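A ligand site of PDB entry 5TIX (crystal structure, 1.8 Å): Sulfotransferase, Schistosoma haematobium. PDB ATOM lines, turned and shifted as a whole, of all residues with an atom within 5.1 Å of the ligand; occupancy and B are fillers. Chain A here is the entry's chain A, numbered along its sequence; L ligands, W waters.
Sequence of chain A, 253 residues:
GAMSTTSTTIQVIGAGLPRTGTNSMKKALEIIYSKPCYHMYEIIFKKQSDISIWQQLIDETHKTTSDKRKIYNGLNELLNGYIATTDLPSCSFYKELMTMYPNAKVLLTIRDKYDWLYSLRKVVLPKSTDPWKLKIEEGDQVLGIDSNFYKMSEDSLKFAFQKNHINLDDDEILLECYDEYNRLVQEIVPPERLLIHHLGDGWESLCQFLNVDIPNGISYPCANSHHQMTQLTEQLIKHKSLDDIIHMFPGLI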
ATOM      1  N   LEU A  17      23.701 -38.803   8.547  1.00  0.00           N
ATOM      2  CA  LEU A  17      23.507 -38.755   9.991  1.00  0.00           C
ATOM      3  C   LEU A  17      22.931 -37.411  10.416  1.00  0.00           C
ATOM      4  O   LEU A  17      22.959 -36.440   9.645  1.00  0.00           O
ATOM      5  CB  LEU A  17      24.844 -38.991  10.685  1.00  0.00           C
ATOM      6  CG  LEU A  17      25.428 -40.399  10.515  1.00  0.00           C
ATOM      7  CD1 LEU A  17      26.891 -40.436  10.945  1.00  0.00           C
ATOM      8  CD2 LEU A  17      24.622 -41.400  11.318  1.00  0.00           C
ATOM      9  N   PRO A  18      22.376 -37.318  11.626  1.00  0.00           N
ATOM     10  CA  PRO A  18      21.872 -36.018  12.081  1.00  0.00           C
ATOM     11  C   PRO A  18      22.964 -34.959  12.059  1.00  0.00           C
ATOM     12  O   PRO A  18      24.160 -35.252  12.238  1.00  0.00           O
ATOM     13  CB  PRO A  18      21.383 -36.297  13.507  1.00  0.00           C
ATOM     14  CG  PRO A  18      21.936 -37.618  13.885  1.00  0.00           C
ATOM     15  CD  PRO A  18      22.102 -38.375  12.607  1.00  0.00           C
ATOM     16  N   ARG A  19      22.542 -33.725  11.826  1.00  0.00           N
ATOM     17  CA  ARG A  19      23.402 -32.549  11.767  1.00  0.00           C
ATOM     18  C   ARG A  19      24.276 -32.501  10.517  1.00  0.00           C
ATOM     19  O   ARG A  19      25.325 -31.838  10.520  1.00  0.00           O
ATOM     20  CB  ARG A  19      24.245 -32.386  13.040  1.00  0.00           C
ATOM     21  CG  ARG A  19      23.444 -32.485  14.337  1.00  0.00           C
ATOM     22  CD  ARG A  19      22.201 -31.606  14.342  1.00  0.00           C
ATOM     23  NE  ARG A  19      22.504 -30.179  14.229  1.00  0.00           N
ATOM     24  CZ  ARG A  19      21.586 -29.234  14.051  1.00  0.00           C
ATOM     25  NH1 ARG A  19      20.308 -29.551  13.949  1.00  0.00           N
ATOM     26  NH2 ARG A  19      21.945 -27.956  13.977  1.00  0.00           N
ATOM     27  N   THR A  20      23.861 -33.159   9.423  1.00  0.00           N
ATOM     28  CA  THR A  20      24.565 -33.106   8.139  1.00  0.00           C
ATOM     29  C   THR A  20      23.713 -32.445   7.065  1.00  0.00           C
ATOM     30  O   THR A  20      24.016 -32.586   5.876  1.00  0.00           O
ATOM     31  CB  THR A  20      24.982 -34.504   7.682  1.00  0.00           C
ATOM     32  OG1 THR A  20      23.815 -35.312   7.459  1.00  0.00           O
ATOM     33  CG2 THR A  20      25.892 -35.182   8.699  1.00  0.00           C
ATOM     34  N   GLY A  21      22.661 -31.749   7.455  1.00  0.00           N
ATOM     35  CA  GLY A  21      21.746 -31.132   6.513  1.00  0.00           C
ATOM     36  C   GLY A  21      20.509 -31.940   6.191  1.00  0.00           C
ATOM     37  O   GLY A  21      19.928 -31.722   5.126  1.00  0.00           O
ATOM     38  N   THR A  22      20.080 -32.838   7.076  1.00  0.00           N
ATOM     39  CA  THR A  22      18.960 -33.721   6.759  1.00  0.00           C
ATOM     40  C   THR A  22      17.654 -32.945   6.660  1.00  0.00           C
ATOM     41  O   THR A  22      16.788 -33.292   5.835  1.00  0.00           O
ATOM     42  CB  THR A  22      18.859 -34.840   7.787  1.00  0.00           C
ATOM     43  OG1 THR A  22      18.633 -34.289   9.087  1.00  0.00           O
ATOM     44  CG2 THR A  22      20.141 -35.671   7.802  1.00  0.00           C
ATOM     45  N   ASN A  23      17.464 -31.912   7.477  1.00  0.00           N
ATOM     46  CA  ASN A  23      16.215 -31.153   7.427  1.00  0.00           C
ATOM     47  C   ASN A  23      16.109 -30.361   6.136  1.00  0.00           C
ATOM     48  O   ASN A  23      15.021 -30.285   5.543  1.00  0.00           O
ATOM     49  CB  ASN A  23      16.077 -30.240   8.643  1.00  0.00           C
ATOM     50  CG  ASN A  23      14.674 -29.708   8.814  1.00  0.00           C
ATOM     51  OD1 ASN A  23      14.379 -28.571   8.433  1.00  0.00           O
ATOM     52  ND2 ASN A  23      13.785 -30.544   9.343  1.00  0.00           N
ATOM     53  N   SER A  24      17.201 -29.756   5.691  1.00  0.00           N
ATOM     54  CA  SER A  24      17.193 -29.069   4.400  1.00  0.00           C
ATOM     55  C   SER A  24      16.937 -30.064   3.267  1.00  0.00           C
ATOM     56  O   SER A  24      16.187 -29.763   2.332  1.00  0.00           O
ATOM     57  CB  SER A  24      18.516 -28.325   4.209  1.00  0.00           C
ATOM     58  OG  SER A  24      18.599 -27.247   5.116  1.00  0.00           O
ATOM     59  N   HIS A  39      11.450 -37.449   8.724  1.00  0.00           N
ATOM     60  CA  HIS A  39      12.565 -36.822   9.429  1.00  0.00           C
ATOM     61  C   HIS A  39      12.297 -37.001  10.919  1.00  0.00           C
ATOM     62  O   HIS A  39      11.185 -37.339  11.323  1.00  0.00           O
ATOM     63  CB  HIS A  39      12.661 -35.330   9.077  1.00  0.00           C
ATOM     64  CG  HIS A  39      13.910 -34.652   9.578  1.00  0.00           C
ATOM     65  ND1 HIS A  39      13.954 -33.949  10.769  1.00  0.00           N
ATOM     66  CD2 HIS A  39      15.142 -34.539   9.037  1.00  0.00           C
ATOM     67  CE1 HIS A  39      15.159 -33.461  10.949  1.00  0.00           C
ATOM     68  NE2 HIS A  39      15.902 -33.800   9.904  1.00  0.00           N
ATOM     69  N   ASP A  87      17.505 -38.430   8.138  1.00  0.00           N
ATOM     70  CA  ASP A  87      17.853 -38.317   9.552  1.00  0.00           C
ATOM     71  C   ASP A  87      17.695 -39.646  10.284  1.00  0.00           C
ATOM     72  O   ASP A  87      17.220 -40.632   9.705  1.00  0.00           O
ATOM     73  CB  ASP A  87      17.011 -37.231  10.236  1.00  0.00           C
ATOM     74  CG  ASP A  87      17.663 -36.667  11.495  1.00  0.00           C
ATOM     75  OD1 ASP A  87      18.693 -37.225  11.942  1.00  0.00           O
ATOM     76  OD2 ASP A  87      17.139 -35.679  12.054  1.00  0.00           O
ATOM     77  N   ARG A 111      29.439 -33.638   5.710  1.00  0.00           N
ATOM     78  CA  ARG A 111      30.049 -32.352   5.998  1.00  0.00           C
ATOM     79  C   ARG A 111      31.364 -32.591   6.728  1.00  0.00           C
ATOM     80  O   ARG A 111      31.703 -33.725   7.084  1.00  0.00           O
ATOM     81  CB  ARG A 111      29.125 -31.475   6.847  1.00  0.00           C
ATOM     82  CG  ARG A 111      29.102 -31.865   8.316  1.00  0.00           C
ATOM     83  CD  ARG A 111      28.049 -31.112   9.096  1.00  0.00           C
ATOM     84  NE  ARG A 111      28.378 -29.704   9.294  1.00  0.00           N
ATOM     85  CZ  ARG A 111      27.676 -28.868  10.048  1.00  0.00           C
ATOM     86  NH1 ARG A 111      26.594 -29.303  10.693  1.00  0.00           N
ATOM     87  NH2 ARG A 111      28.041 -27.605  10.174  1.00  0.00           N
ATOM     88  N   ASP A 115      33.004 -29.777  12.231  1.00  0.00           N
ATOM     89  CA  ASP A 115      31.754 -29.028  12.271  1.00  0.00           C
ATOM     90  C   ASP A 115      30.592 -29.920  12.693  1.00  0.00           C
ATOM     91  O   ASP A 115      29.713 -29.498  13.442  1.00  0.00           O
ATOM     92  CB  ASP A 115      31.467 -28.416  10.908  1.00  0.00           C
ATOM     93  CG  ASP A 115      32.494 -27.371  10.501  1.00  0.00           C
ATOM     94  OD1 ASP A 115      33.209 -26.873  11.389  1.00  0.00           O
ATOM     95  OD2 ASP A 115      32.567 -27.054   9.295  1.00  0.00           O
ATOM     96  N   SER A 119      28.161 -29.439  16.053  1.00  0.00           N
ATOM     97  CA  SER A 119      26.719 -29.310  15.897  1.00  0.00           C
ATOM     98  C   SER A 119      25.973 -30.371  16.707  1.00  0.00           C
ATOM     99  O   SER A 119      24.940 -30.107  17.313  1.00  0.00           O
ATOM    100  CB  SER A 119      26.358 -29.431  14.417  1.00  0.00           C
ATOM    101  OG  SER A 119      24.993 -29.149  14.179  1.00  0.00           O
ATOM    102  N   LEU A 199      27.555 -30.366   2.303  1.00  0.00           N
ATOM    103  CA  LEU A 199      26.852 -29.187   2.780  1.00  0.00           C
ATOM    104  C   LEU A 199      27.168 -28.004   1.875  1.00  0.00           C
ATOM    105  O   LEU A 199      28.331 -27.705   1.604  1.00  0.00           O
ATOM    106  CB  LEU A 199      27.276 -28.904   4.219  1.00  0.00           C
ATOM    107  CG  LEU A 199      26.245 -28.316   5.188  1.00  0.00           C
ATOM    108  CD1 LEU A 199      24.918 -29.078   5.153  1.00  0.00           C
ATOM    109  CD2 LEU A 199      26.826 -28.330   6.598  1.00  0.00           C
ATOM    110  N   GLY A 200      26.119 -27.335   1.392  1.00  0.00           N
ATOM    111  CA  GLY A 200      26.262 -26.230   0.470  1.00  0.00           C
ATOM    112  C   GLY A 200      26.211 -26.602  -1.003  1.00  0.00           C
ATOM    113  O   GLY A 200      26.322 -25.699  -1.846  1.00  0.00           O
ATOM    114  N   TYR A 220      17.724 -23.343  -2.516  1.00  0.00           N
ATOM    115  CA  TYR A 220      17.894 -24.581  -1.757  1.00  0.00           C
ATOM    116  C   TYR A 220      17.715 -24.303  -0.270  1.00  0.00           C
ATOM    117  O   TYR A 220      18.276 -23.337   0.243  1.00  0.00           O
ATOM    118  CB  TYR A 220      19.273 -25.185  -2.013  1.00  0.00           C
ATOM    119  CG  TYR A 220      19.409 -26.567  -1.401  1.00  0.00           C
ATOM    120  CD1 TYR A 220      19.029 -27.699  -2.108  1.00  0.00           C
ATOM    121  CD2 TYR A 220      19.871 -26.727  -0.105  1.00  0.00           C
ATOM    122  CE1 TYR A 220      19.130 -28.960  -1.539  1.00  0.00           C
ATOM    123  CE2 TYR A 220      19.980 -27.976   0.469  1.00  0.00           C
ATOM    124  CZ  TYR A 220      19.606 -29.095  -0.259  1.00  0.00           C
ATOM    125  OH  TYR A 220      19.707 -30.344   0.303  1.00  0.00           O
ATOM    126  N   PRO A 221      16.943 -25.124   0.445  1.00  0.00           N
ATOM    127  CA  PRO A 221      16.651 -24.819   1.851  1.00  0.00           C
ATOM    128  C   PRO A 221      17.913 -24.736   2.707  1.00  0.00           C
ATOM    129  O   PRO A 221      18.906 -25.408   2.465  1.00  0.00           O
ATOM    130  CB  PRO A 221      15.751 -25.976   2.299  1.00  0.00           C
ATOM    131  CG  PRO A 221      15.153 -26.496   1.027  1.00  0.00           C
ATOM    132  CD  PRO A 221      16.217 -26.333  -0.003  1.00  0.00           C
ATOM    133  N   CYS A 222      17.830 -23.888   3.753  1.00  0.00           N
ATOM    134  CA  CYS A 222      18.934 -23.650   4.692  1.00  0.00           C
ATOM    135  C   CYS A 222      18.302 -23.605   6.084  1.00  0.00           C
ATOM    136  O   CYS A 222      18.093 -22.544   6.669  1.00  0.00           O
ATOM    137  CB  CYS A 222      19.671 -22.362   4.356  1.00  0.00           C
ATOM    138  SG  CYS A 222      21.345 -22.267   5.043  1.00  0.00           S
ATOM    139  N   ALA A 223      17.990 -24.787   6.621  1.00  0.00           N
ATOM    140  CA  ALA A 223      17.176 -24.894   7.827  1.00  0.00           C
ATOM    141  C   ALA A 223      17.936 -25.585   8.952  1.00  0.00           C
ATOM    142  O   ALA A 223      18.897 -26.323   8.728  1.00  0.00           O
ATOM    143  CB  ALA A 223      15.896 -25.704   7.529  1.00  0.00           C
ATOM    144  N   ASN A 224      17.492 -25.303  10.177  1.00  0.00           N
ATOM    145  CA  ASN A 224      17.848 -26.121  11.341  1.00  0.00           C
ATOM    146  C   ASN A 224      19.269 -25.904  11.857  1.00  0.00           C
ATOM    147  O   ASN A 224      19.938 -26.872  12.240  1.00  0.00           O
ATOM    148  CB  ASN A 224      17.645 -27.590  10.974  1.00  0.00           C
ATOM    149  CG  ASN A 224      17.459 -28.480  12.185  1.00  0.00           C
ATOM    150  OD1 ASN A 224      17.048 -28.009  13.255  1.00  0.00           O
ATOM    151  ND2 ASN A 224      17.746 -29.766  12.030  1.00  0.00           N
ATOM    152  N   SER A 225      19.743 -24.666  11.896  1.00  0.00           N
ATOM    153  CA  SER A 225      21.068 -24.385  12.427  1.00  0.00           C
ATOM    154  C   SER A 225      21.075 -24.539  13.948  1.00  0.00           C
ATOM    155  O   SER A 225      20.041 -24.393  14.618  1.00  0.00           O
ATOM    156  CB  SER A 225      21.487 -22.962  12.062  1.00  0.00           C
ATOM    157  OG  SER A 225      20.729 -22.006  12.785  1.00  0.00           O
ATOM    158  N   HIS A 226      22.253 -24.828  14.503  1.00  0.00           N
ATOM    159  CA  HIS A 226      22.331 -24.975  15.952  1.00  0.00           C
ATOM    160  C   HIS A 226      22.015 -23.665  16.658  1.00  0.00           C
ATOM    161  O   HIS A 226      21.515 -23.664  17.787  1.00  0.00           O
ATOM    162  CB  HIS A 226      23.700 -25.531  16.376  1.00  0.00           C
ATOM    163  CG  HIS A 226      24.833 -24.552  16.265  1.00  0.00           C
ATOM    164  ND1 HIS A 226      25.012 -23.521  17.158  1.00  0.00           N
ATOM    165  CD2 HIS A 226      25.843 -24.456  15.370  1.00  0.00           C
ATOM    166  CE1 HIS A 226      26.084 -22.835  16.815  1.00  0.00           C
ATOM    167  NE2 HIS A 226      26.605 -23.381  15.738  1.00  0.00           N
ATOM    168  N   HIS A 227      22.296 -22.531  16.008  1.00  0.00           N
ATOM    169  CA  HIS A 227      21.898 -21.248  16.575  1.00  0.00           C
ATOM    170  C   HIS A 227      20.383 -21.155  16.735  1.00  0.00           C
ATOM    171  O   HIS A 227      19.889 -20.710  17.771  1.00  0.00           O
ATOM    172  CB  HIS A 227      22.407 -20.107  15.681  1.00  0.00           C
ATOM    173  CG  HIS A 227      21.964 -18.751  16.128  1.00  0.00           C
ATOM    174  ND1 HIS A 227      22.480 -18.124  17.245  1.00  0.00           N
ATOM    175  CD2 HIS A 227      21.047 -17.895  15.615  1.00  0.00           C
ATOM    176  CE1 HIS A 227      21.900 -16.940  17.392  1.00  0.00           C
ATOM    177  NE2 HIS A 227      21.024 -16.782  16.412  1.00  0.00           N
HETATM  178  P1  LIG L   1      24.976 -26.094  12.141  1.00  0.00           P
HETATM  179  O1  LIG L   1      26.482 -26.052  12.166  1.00  0.00           O
HETATM  180  O2  LIG L   1      24.456 -26.694  13.448  1.00  0.00           O
HETATM  181  O3  LIG L   1      24.430 -24.686  11.980  1.00  0.00           O
HETATM  182  P2  LIG L   1      20.342 -31.429  10.318  1.00  0.00           P
HETATM  183  O4  LIG L   1      20.625 -32.832   9.823  1.00  0.00           O
HETATM  184  O5  LIG L   1      19.082 -30.903   9.692  1.00  0.00           O
HETATM  185  O6  LIG L   1      20.180 -31.458  11.824  1.00  0.00           O
HETATM  186  O7  LIG L   1      21.557 -30.467   9.924  1.00  0.00           O
HETATM  187  C1  LIG L   1      21.610 -29.135  10.455  1.00  0.00           C
HETATM  188  C2  LIG L   1      22.951 -28.573  10.096  1.00  0.00           C
HETATM  189  O8  LIG L   1      23.093 -28.439   8.653  1.00  0.00           O
HETATM  190  C3  LIG L   1      23.123 -27.202  10.642  1.00  0.00           C
HETATM  191  O9  LIG L   1      24.504 -26.992  10.912  1.00  0.00           O
HETATM  192  C4  LIG L   1      22.672 -26.349   9.523  1.00  0.00           C
HETATM  193  O10 LIG L   1      23.162 -25.028   9.653  1.00  0.00           O
HETATM  194  C5  LIG L   1      23.294 -27.054   8.362  1.00  0.00           C
HETATM  195  N1  LIG L   1      22.715 -26.718   7.127  1.00  0.00           N
HETATM  196  C6  LIG L   1      21.460 -27.020   6.743  1.00  0.00           C
HETATM  197  N2  LIG L   1      21.251 -26.560   5.505  1.00  0.00           N
HETATM  198  C7  LIG L   1      22.391 -25.941   5.065  1.00  0.00           C
HETATM  199  C8  LIG L   1      22.787 -25.278   3.854  1.00  0.00           C
HETATM  200  N3  LIG L   1      21.878 -25.147   2.795  1.00  0.00           N
HETATM  201  N4  LIG L   1      24.030 -24.780   3.769  1.00  0.00           N
HETATM  202  C9  LIG L   1      24.889 -24.894   4.767  1.00  0.00           C
HETATM  203  N5  LIG L   1      24.570 -25.509   5.904  1.00  0.00           N
HETATM  204  C10 LIG L   1      23.336 -26.058   6.105  1.00  0.00           C
HETATM  205  O   HOH W   1      24.829 -22.660   2.063  1.00  0.00           O
HETATM  206  O   HOH W   2      26.679 -24.507   7.824  1.00  0.00           O
HETATM  207  O   HOH W   3      19.216 -28.994   7.677  1.00  0.00           O
HETATM  208  O   HOH W   4      21.632 -23.276   8.389  1.00  0.00           O
HETATM  209  O   HOH W   5      25.135 -22.060  11.467  1.00  0.00           O
HETATM  210  O   HOH W   6      27.475 -24.132  10.526  1.00  0.00           O
HETATM  211  O   HOH W   7      17.856 -32.994  12.843  1.00  0.00           O
HETATM  212  O   HOH W   8      22.472 -24.072   0.096  1.00  0.00           O
HETATM  213  O   HOH W   9      28.854 -26.753  13.687  1.00  0.00           O
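An oxygen (O4) of the ligand lies within hydrogen-bond range of the backbone NH of Thr 22 (2.8 Å). O4 of the ligand lies within hydrogen-bond range of OG1 of Thr 22, 2.6 Å away. The side-chain hydroxyl (OG) of Ser 119 sits at hydrogen-bond distance from an oxygen (O2) of the ligand (2.6 Å). The side-chain hydroxyl (OG) of Ser 24 sits at hydrogen-bond distance from a nitrogen (N2) of the ligand, at 2.8 Å. The backbone NH of Arg 19 is in hydrogen-bond range of an oxygen (O4) of the ligand (2.9 Å). O6 of the ligand is in salt-bridge range of NH1 of Arg 19 (2.9 Å). The backbone NH of Asn 23 is in hydrogen-bond range of an oxygen (O5) of the ligand. ND2 of Asn 224 lies within hydrogen-bond range of O5 of the ligand (2.9 Å). An oxygen (O1) of the ligand lies within salt-bridge range of the guanidinium group (NH2) of Arg 111 (3.0 Å). N of Gly 21 is in hydrogen-bond range of O7 of the ligand (3.0 Å). The backbone carbonyl oxygen of Pro 221 sits at hydrogen-bond distance from a nitrogen (N3) of the ligand (3.0 Å). O2 of the ligand is in hydrogen-bond range of N of His 226 (3.1 Å). N of Thr 20 is in hydrogen-bond range of O4 of the ligand. SG of Cys 222 sits close to N3 of the ligand, at 3.7 Å.
NE2 of His 39 lies within hydrogen-bond range of OG1 of Thr 22 (2.9 Å). OG of Ser 119 is in hydrogen-bond range of NE of Arg 19. The side-chain hydroxyl (OG) of Ser 24 sits at hydrogen-bond distance from the backbone carbonyl oxygen (O) of Pro 221, 3.2 Å away. OG of Ser 24 lies within hydrogen-bond range of N of Ala 223 (2.9 Å). The guanidinium group (NH2) of Arg 19 is in hydrogen-bond range of the backbone carbonyl oxygen (O) of Asn 224 (2.9 Å). The backbone carbonyl oxygen of Arg 19 sits at hydrogen-bond distance from the guanidinium group of Arg 111, at 2.8 Å. NE2 of His 39 lies within hydrogen-bond range of N of Asn 23 (3.4 Å). The backbone carbonyl oxygen of Leu 17 lies within hydrogen-bond range of the side-chain hydroxyl of Thr 20 (2.6 Å).
Merely in contact with the ligand: Pro 18 (3.9 Å), Leu 199 (3.3 Å), Tyr 220 (3.9 Å), Ala 223 (3.3 Å) and Ser 225 (3.4 Å). Of the 23 residues printed, 17 come within 4 Å of the ligand.
Water W4 bridges O10 of the ligand (2.6 Å) and SG of Cys 222 (3.5 Å). Water W3 lies within hydrogen-bond range of O5 of the ligand, O of Ala 223, N of Ser 24 and N of Asn 23. Water W9 lies within hydrogen-bond range of the backbone carbonyl oxygen of Asp 115 and an oxygen (O1) of the ligand. Water W7 lies within hydrogen-bond range of the side-chain carboxylate (OD2) of Asp 87 (2.9 Å), an oxygen (O6) of the ligand (3.0 Å) and the side-chain amide nitrogen (ND2) of Asn 224 (3.3 Å).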
